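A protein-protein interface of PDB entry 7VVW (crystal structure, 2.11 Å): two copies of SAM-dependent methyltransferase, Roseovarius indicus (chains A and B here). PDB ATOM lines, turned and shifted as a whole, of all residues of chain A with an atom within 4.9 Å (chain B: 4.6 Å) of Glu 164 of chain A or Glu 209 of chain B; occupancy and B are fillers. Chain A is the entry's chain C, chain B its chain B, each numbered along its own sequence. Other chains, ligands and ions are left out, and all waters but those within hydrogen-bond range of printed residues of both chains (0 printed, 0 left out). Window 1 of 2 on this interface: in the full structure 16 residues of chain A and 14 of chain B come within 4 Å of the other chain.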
ATOM      1  N   PRO A 161      -5.760 -12.296  29.693  1.00  0.00           N
ATOM      2  CA  PRO A 161      -6.479 -12.494  28.449  1.00  0.00           C
ATOM      3  C   PRO A 161      -7.830 -12.986  28.683  1.00  0.00           C
ATOM      4  O   PRO A 161      -8.082 -13.559  29.677  1.00  0.00           O
ATOM      5  CB  PRO A 161      -5.632 -13.501  27.740  1.00  0.00           C
ATOM      6  CG  PRO A 161      -5.372 -14.432  28.814  1.00  0.00           C
ATOM      7  CD  PRO A 161      -4.984 -13.581  29.947  1.00  0.00           C
ATOM      8  N   TRP A 162      -8.674 -12.738  27.736  1.00  0.00           N
ATOM      9  CA  TRP A 162     -10.016 -13.077  27.887  1.00  0.00           C
ATOM     10  C   TRP A 162     -10.365 -13.892  26.708  1.00  0.00           C
ATOM     11  O   TRP A 162     -11.279 -14.636  26.714  1.00  0.00           O
ATOM     12  CB  TRP A 162     -10.786 -11.720  27.923  1.00  0.00           C
ATOM     13  CG  TRP A 162     -12.048 -11.528  28.863  1.00  0.00           C
ATOM     14  CD1 TRP A 162     -13.276 -11.064  28.482  1.00  0.00           C
ATOM     15  CD2 TRP A 162     -12.167 -11.799  30.284  1.00  0.00           C
ATOM     16  NE1 TRP A 162     -14.132 -11.038  29.551  1.00  0.00           N
ATOM     17  CE2 TRP A 162     -13.471 -11.480  30.665  1.00  0.00           C
ATOM     18  CE3 TRP A 162     -11.308 -12.288  31.255  1.00  0.00           C
ATOM     19  CZ2 TRP A 162     -13.906 -11.651  31.953  1.00  0.00           C
ATOM     20  CZ3 TRP A 162     -11.764 -12.417  32.514  1.00  0.00           C
ATOM     21  CH2 TRP A 162     -13.021 -12.111  32.851  1.00  0.00           C
ATOM     22  N   ALA A 163      -9.640 -13.763  25.662  1.00  0.00           N
ATOM     23  CA  ALA A 163     -10.122 -14.482  24.490  1.00  0.00           C
ATOM     24  C   ALA A 163     -10.202 -15.965  24.544  1.00  0.00           C
ATOM     25  O   ALA A 163     -11.085 -16.506  24.064  1.00  0.00           O
ATOM     26  CB  ALA A 163      -9.421 -14.074  23.264  1.00  0.00           C
ATOM     27  N   GLU A 164      -9.232 -16.610  25.100  1.00  0.00           N
ATOM     28  CA  GLU A 164      -9.278 -18.068  25.105  1.00  0.00           C
ATOM     29  C   GLU A 164     -10.371 -18.607  26.014  1.00  0.00           C
ATOM     30  O   GLU A 164     -10.736 -19.782  25.896  1.00  0.00           O
ATOM     31  CB  GLU A 164      -7.925 -18.643  25.534  1.00  0.00           C
ATOM     32  CG  GLU A 164      -7.474 -18.189  26.900  1.00  0.00           C
ATOM     33  CD  GLU A 164      -6.349 -17.186  26.831  1.00  0.00           C
ATOM     34  OE1 GLU A 164      -5.345 -17.384  27.548  1.00  0.00           O
ATOM     35  OE2 GLU A 164      -6.461 -16.204  26.064  1.00  0.00           O
ATOM     36  N   PHE A 165     -10.895 -17.785  26.918  1.00  0.00           N
ATOM     37  CA  PHE A 165     -11.977 -18.195  27.793  1.00  0.00           C
ATOM     38  C   PHE A 165     -13.342 -17.886  27.207  1.00  0.00           C
ATOM     39  O   PHE A 165     -14.356 -18.118  27.871  1.00  0.00           O
ATOM     40  CB  PHE A 165     -11.807 -17.537  29.160  1.00  0.00           C
ATOM     41  CG  PHE A 165     -10.430 -17.710  29.722  1.00  0.00           C
ATOM     42  CD1 PHE A 165      -9.937 -18.977  29.997  1.00  0.00           C
ATOM     43  CD2 PHE A 165      -9.602 -16.618  29.923  1.00  0.00           C
ATOM     44  CE1 PHE A 165      -8.659 -19.150  30.492  1.00  0.00           C
ATOM     45  CE2 PHE A 165      -8.330 -16.782  30.419  1.00  0.00           C
ATOM     46  CZ  PHE A 165      -7.852 -18.054  30.702  1.00  0.00           C
ATOM     47  N   ASP A 166     -13.390 -17.395  25.969  1.00  0.00           N
ATOM     48  CA  ASP A 166     -14.639 -16.907  25.402  1.00  0.00           C
ATOM     49  C   ASP A 166     -15.585 -18.027  25.001  1.00  0.00           C
ATOM     50  O   ASP A 166     -16.779 -17.774  24.853  1.00  0.00           O
ATOM     51  CB  ASP A 166     -14.355 -16.021  24.184  1.00  0.00           C
ATOM     52  CG  ASP A 166     -15.621 -15.422  23.581  1.00  0.00           C
ATOM     53  OD1 ASP A 166     -16.316 -14.667  24.286  1.00  0.00           O
ATOM     54  OD2 ASP A 166     -15.927 -15.723  22.407  1.00  0.00           O
ATOM     55  N   SER A 167     -15.076 -19.244  24.791  1.00  0.00           N
ATOM     56  CA  SER A 167     -15.925 -20.332  24.345  1.00  0.00           C
ATOM     57  C   SER A 167     -16.693 -20.979  25.489  1.00  0.00           C
ATOM     58  O   SER A 167     -17.609 -21.759  25.225  1.00  0.00           O
ATOM     59  CB  SER A 167     -15.091 -21.405  23.622  1.00  0.00           C
ATOM     60  OG  SER A 167     -14.451 -22.309  24.527  1.00  0.00           O
ATOM     61  N   TYR A 168     -16.362 -20.668  26.731  1.00  0.00           N
ATOM     62  CA  TYR A 168     -16.937 -21.395  27.848  1.00  0.00           C
ATOM     63  C   TYR A 168     -18.431 -21.124  27.956  1.00  0.00           C
ATOM     64  O   TYR A 168     -18.856 -19.964  27.858  1.00  0.00           O
ATOM     65  CB  TYR A 168     -16.241 -21.012  29.142  1.00  0.00           C
ATOM     66  CG  TYR A 168     -14.978 -21.783  29.339  1.00  0.00           C
ATOM     67  CD1 TYR A 168     -15.015 -23.068  29.857  1.00  0.00           C
ATOM     68  CD2 TYR A 168     -13.750 -21.260  28.949  1.00  0.00           C
ATOM     69  CE1 TYR A 168     -13.862 -23.799  30.027  1.00  0.00           C
ATOM     70  CE2 TYR A 168     -12.585 -21.993  29.106  1.00  0.00           C
ATOM     71  CZ  TYR A 168     -12.658 -23.263  29.657  1.00  0.00           C
ATOM     72  OH  TYR A 168     -11.537 -24.012  29.844  1.00  0.00           O
ATOM     73  N   ALA A 180     -13.192 -21.989  33.540  1.00  0.00           N
ATOM     74  CA  ALA A 180     -11.898 -22.508  33.112  1.00  0.00           C
ATOM     75  C   ALA A 180     -11.133 -23.091  34.288  1.00  0.00           C
ATOM     76  O   ALA A 180     -10.529 -24.162  34.177  1.00  0.00           O
ATOM     77  CB  ALA A 180     -11.081 -21.398  32.432  1.00  0.00           C
ATOM     78  N   ARG A 184      -9.907 -27.249  35.384  1.00  0.00           N
ATOM     79  CA  ARG A 184      -8.541 -27.605  35.737  1.00  0.00           C
ATOM     80  C   ARG A 184      -8.484 -28.240  37.112  1.00  0.00           C
ATOM     81  O   ARG A 184      -7.741 -29.211  37.320  1.00  0.00           O
ATOM     82  CB  ARG A 184      -7.637 -26.366  35.692  1.00  0.00           C
ATOM     83  CG  ARG A 184      -7.373 -25.808  34.301  1.00  0.00           C
ATOM     84  CD  ARG A 184      -7.064 -24.284  34.356  1.00  0.00           C
ATOM     85  NE  ARG A 184      -6.404 -23.792  33.146  1.00  0.00           N
ATOM     86  CZ  ARG A 184      -7.035 -23.515  32.008  1.00  0.00           C
ATOM     87  NH1 ARG A 184      -8.354 -23.672  31.909  1.00  0.00           N
ATOM     88  NH2 ARG A 184      -6.354 -23.080  30.959  1.00  0.00           N
ATOM     89  N   PHE B 170     -15.869 -25.328  21.666  1.00  0.00           N
ATOM     90  CA  PHE B 170     -14.759 -24.981  20.782  1.00  0.00           C
ATOM     91  C   PHE B 170     -15.109 -25.081  19.306  1.00  0.00           C
ATOM     92  O   PHE B 170     -14.241 -24.822  18.460  1.00  0.00           O
ATOM     93  CB  PHE B 170     -13.529 -25.832  21.108  1.00  0.00           C
ATOM     94  CG  PHE B 170     -12.838 -25.368  22.350  1.00  0.00           C
ATOM     95  CD1 PHE B 170     -13.292 -25.778  23.595  1.00  0.00           C
ATOM     96  CD2 PHE B 170     -11.800 -24.440  22.277  1.00  0.00           C
ATOM     97  CE1 PHE B 170     -12.681 -25.321  24.749  1.00  0.00           C
ATOM     98  CE2 PHE B 170     -11.190 -23.973  23.416  1.00  0.00           C
ATOM     99  CZ  PHE B 170     -11.622 -24.410  24.654  1.00  0.00           C
ATOM    100  N   ALA B 205      -2.967 -19.914  22.437  1.00  0.00           N
ATOM    101  CA  ALA B 205      -3.743 -19.827  23.668  1.00  0.00           C
ATOM    102  C   ALA B 205      -5.058 -20.586  23.517  1.00  0.00           C
ATOM    103  O   ALA B 205      -5.425 -21.404  24.373  1.00  0.00           O
ATOM    104  CB  ALA B 205      -3.991 -18.360  24.042  1.00  0.00           C
ATOM    105  N   VAL B 206      -5.748 -20.377  22.394  1.00  0.00           N
ATOM    106  CA  VAL B 206      -7.018 -21.055  22.170  1.00  0.00           C
ATOM    107  C   VAL B 206      -6.792 -22.547  21.975  1.00  0.00           C
ATOM    108  O   VAL B 206      -7.535 -23.369  22.519  1.00  0.00           O
ATOM    109  CB  VAL B 206      -7.760 -20.432  20.977  1.00  0.00           C
ATOM    110  CG1 VAL B 206      -9.002 -21.249  20.656  1.00  0.00           C
ATOM    111  CG2 VAL B 206      -8.134 -18.982  21.295  1.00  0.00           C
ATOM    112  N   LEU B 207      -5.758 -22.922  21.209  1.00  0.00           N
ATOM    113  CA  LEU B 207      -5.464 -24.339  21.002  1.00  0.00           C
ATOM    114  C   LEU B 207      -5.174 -25.045  22.326  1.00  0.00           C
ATOM    115  O   LEU B 207      -5.646 -26.167  22.555  1.00  0.00           O
ATOM    116  CB  LEU B 207      -4.288 -24.495  20.036  1.00  0.00           C
ATOM    117  CG  LEU B 207      -4.492 -24.092  18.566  1.00  0.00           C
ATOM    118  CD1 LEU B 207      -3.289 -24.516  17.683  1.00  0.00           C
ATOM    119  CD2 LEU B 207      -5.776 -24.686  18.019  1.00  0.00           C
ATOM    120  N   PHE B 208      -4.431 -24.391  23.224  1.00  0.00           N
ATOM    121  CA  PHE B 208      -4.109 -25.011  24.504  1.00  0.00           C
ATOM    122  C   PHE B 208      -5.356 -25.133  25.382  1.00  0.00           C
ATOM    123  O   PHE B 208      -5.532 -26.130  26.100  1.00  0.00           O
ATOM    124  CB  PHE B 208      -3.012 -24.206  25.209  1.00  0.00           C
ATOM    125  CG  PHE B 208      -1.588 -24.585  24.788  1.00  0.00           C
ATOM    126  CD1 PHE B 208      -1.310 -25.014  23.493  1.00  0.00           C
ATOM    127  CD2 PHE B 208      -0.534 -24.494  25.688  1.00  0.00           C
ATOM    128  CE1 PHE B 208       0.003 -25.361  23.107  1.00  0.00           C
ATOM    129  CE2 PHE B 208       0.785 -24.837  25.311  1.00  0.00           C
ATOM    130  CZ  PHE B 208       1.046 -25.274  24.029  1.00  0.00           C
ATOM    131  N   GLU B 209      -6.240 -24.130  25.324  1.00  0.00           N
ATOM    132  CA  GLU B 209      -7.451 -24.152  26.132  1.00  0.00           C
ATOM    133  C   GLU B 209      -8.358 -25.310  25.741  1.00  0.00           C
ATOM    134  O   GLU B 209      -9.025 -25.891  26.603  1.00  0.00           O
ATOM    135  CB  GLU B 209      -8.196 -22.813  26.013  1.00  0.00           C
ATOM    136  CG  GLU B 209      -9.258 -22.606  27.109  1.00  0.00           C
ATOM    137  CD  GLU B 209      -8.653 -22.583  28.498  1.00  0.00           C
ATOM    138  OE1 GLU B 209      -7.477 -22.222  28.613  1.00  0.00           O
ATOM    139  OE2 GLU B 209      -9.337 -22.943  29.482  1.00  0.00           O
ATOM    140  N   LEU B 210      -8.377 -25.677  24.455  1.00  0.00           N
ATOM    141  CA  LEU B 210      -9.166 -26.824  24.038  1.00  0.00           C
ATOM    142  C   LEU B 210      -8.799 -28.051  24.865  1.00  0.00           C
ATOM    143  O   LEU B 210      -9.675 -28.819  25.277  1.00  0.00           O
ATOM    144  CB  LEU B 210      -8.964 -27.077  22.541  1.00  0.00           C
ATOM    145  CG  LEU B 210      -9.338 -28.453  21.966  1.00  0.00           C
ATOM    146  CD1 LEU B 210     -10.839 -28.606  21.741  1.00  0.00           C
ATOM    147  CD2 LEU B 210      -8.611 -28.691  20.664  1.00  0.00           C
ATOM    148  N   PHE B 211      -7.515 -28.198  25.193  1.00  0.00           N
ATOM    149  CA  PHE B 211      -7.071 -29.328  25.998  1.00  0.00           C
ATOM    150  C   PHE B 211      -7.345 -29.111  27.480  1.00  0.00           C
ATOM    151  O   PHE B 211      -7.833 -30.016  28.167  1.00  0.00           O
ATOM    152  CB  PHE B 211      -5.578 -29.573  25.763  1.00  0.00           C
ATOM    153  CG  PHE B 211      -5.287 -30.198  24.434  1.00  0.00           C
ATOM    154  CD1 PHE B 211      -5.074 -29.402  23.316  1.00  0.00           C
ATOM    155  CD2 PHE B 211      -5.273 -31.589  24.295  1.00  0.00           C
ATOM    156  CE1 PHE B 211      -4.817 -29.965  22.087  1.00  0.00           C
ATOM    157  CE2 PHE B 211      -5.035 -32.159  23.073  1.00  0.00           C
ATOM    158  CZ  PHE B 211      -4.797 -31.355  21.959  1.00  0.00           C
ATOM    159  N   GLU B 212      -7.014 -27.923  27.994  1.00  0.00           N
ATOM    160  CA  GLU B 212      -7.200 -27.656  29.413  1.00  0.00           C
ATOM    161  C   GLU B 212      -8.673 -27.676  29.795  1.00  0.00           C
ATOM    162  O   GLU B 212      -9.016 -28.072  30.909  1.00  0.00           O
ATOM    163  CB  GLU B 212      -6.591 -26.296  29.786  1.00  0.00           C
ATOM    164  CG  GLU B 212      -5.083 -26.215  29.582  1.00  0.00           C
ATOM    165  CD  GLU B 212      -4.303 -26.628  30.820  1.00  0.00           C
ATOM    166  OE1 GLU B 212      -4.925 -27.156  31.784  1.00  0.00           O
ATOM    167  OE2 GLU B 212      -3.066 -26.419  30.819  1.00  0.00           O
ATOM    168  N   ALA B 213      -9.553 -27.224  28.902  1.00  0.00           N
ATOM    169  CA  ALA B 213     -10.987 -27.273  29.178  1.00  0.00           C
ATOM    170  C   ALA B 213     -11.500 -28.705  29.320  1.00  0.00           C
ATOM    171  O   ALA B 213     -12.575 -28.923  29.903  1.00  0.00           O
ATOM    172  CB  ALA B 213     -11.743 -26.565  28.056  1.00  0.00           C
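OH of Tyr 168 of chain A lies within hydrogen-bond range of OE2 of Glu 209 of chain B, at 2.5 Å.
The side-chain carboxylate (OE2) of Glu 209 of chain B is in salt-bridge range of the guanidinium group (NH1) of Arg 184 of chain A (2.7 Å).
The guanidinium group of Arg 184 of chain A is in salt-bridge range of the side-chain carboxylate of Glu 212 of chain B.
O of Ala 180 of chain A sits at hydrogen-bond distance from NH1 of Arg 184 of chain A.
Among the printed residues, pairs that only touch across the chains: Tyr 168 of chain A with Ala 213 of chain B (3.1 Å), Glu 164 of chain A with Glu 209 of chain B (3.4 Å), Ser 167 of chain A with Phe 170 of chain B (3.5 Å), Ala 180 of chain A with Glu 209 of chain B (3.8 Å), Phe 165 of chain A with Glu 209 of chain B (3.8 Å) and Glu 164 of chain A with Ala 205 of chain B (3.8 Å).
Of chain B, only Ala 205 and Glu 209 come within 4 Å of Glu 164 of chain A.
Of chain A, only Glu 164 (3.4 Å), Phe 165 (3.8 Å), Tyr 168 (2.5 Å), Ala 180 (3.8 Å) and Arg 184 (2.7 Å) come within 4 Å of Glu 209 of chain B.
Of the printed residues of chain B, Ala 180 of chain A touches Glu 209.
Of the printed residues of chain B, Tyr 168 of chain A touches Glu 209 (2.5 Å) and Ala 213 (3.1 Å).
Printed residues of chain B within 4 Å of Phe 165 of chain A: Glu 209.
Ala 163 of chain A touches none of the printed residues of chain B.
Asp 166 of chain A touches none of the printed residues of chain B.
The nearest printed residue of chain A that does not touch Ala 205 of chain B is Pro 161 of chain A (6.3 Å).
Of the 10 printed residues of chain A, 6 touch a printed residue of chain B.
Printed residues of chain A that touch a printed residue of chain B: Glu 164, Phe 165, Ser 167, Tyr 168, Ala 180 and Arg 184.
Hydrophobic or aromatic side chains of chain A within 4 Å of the printed part of chain B: Phe 165, Tyr 168 and Ala 180.
Of the 10 printed residues of chain B, 5 touch a printed residue of chain A.
Hydrophobic or aromatic side chains of chain B within 4 Å of the printed part of chain A: Phe 170, Ala 205 and Ala 213.
Among the printed residues, 9 pairs touch across the chains.
Among the printed residues, Asp or Glu carboxylates within 4 Å of a Lys or Arg side-chain nitrogen of the other chain: Arg 184 of chain A with Glu 209 of chain B (2.7 Å) and Arg 184 of chain A with Glu 212 of chain B (3.9 Å).
No position is printed for both chains.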
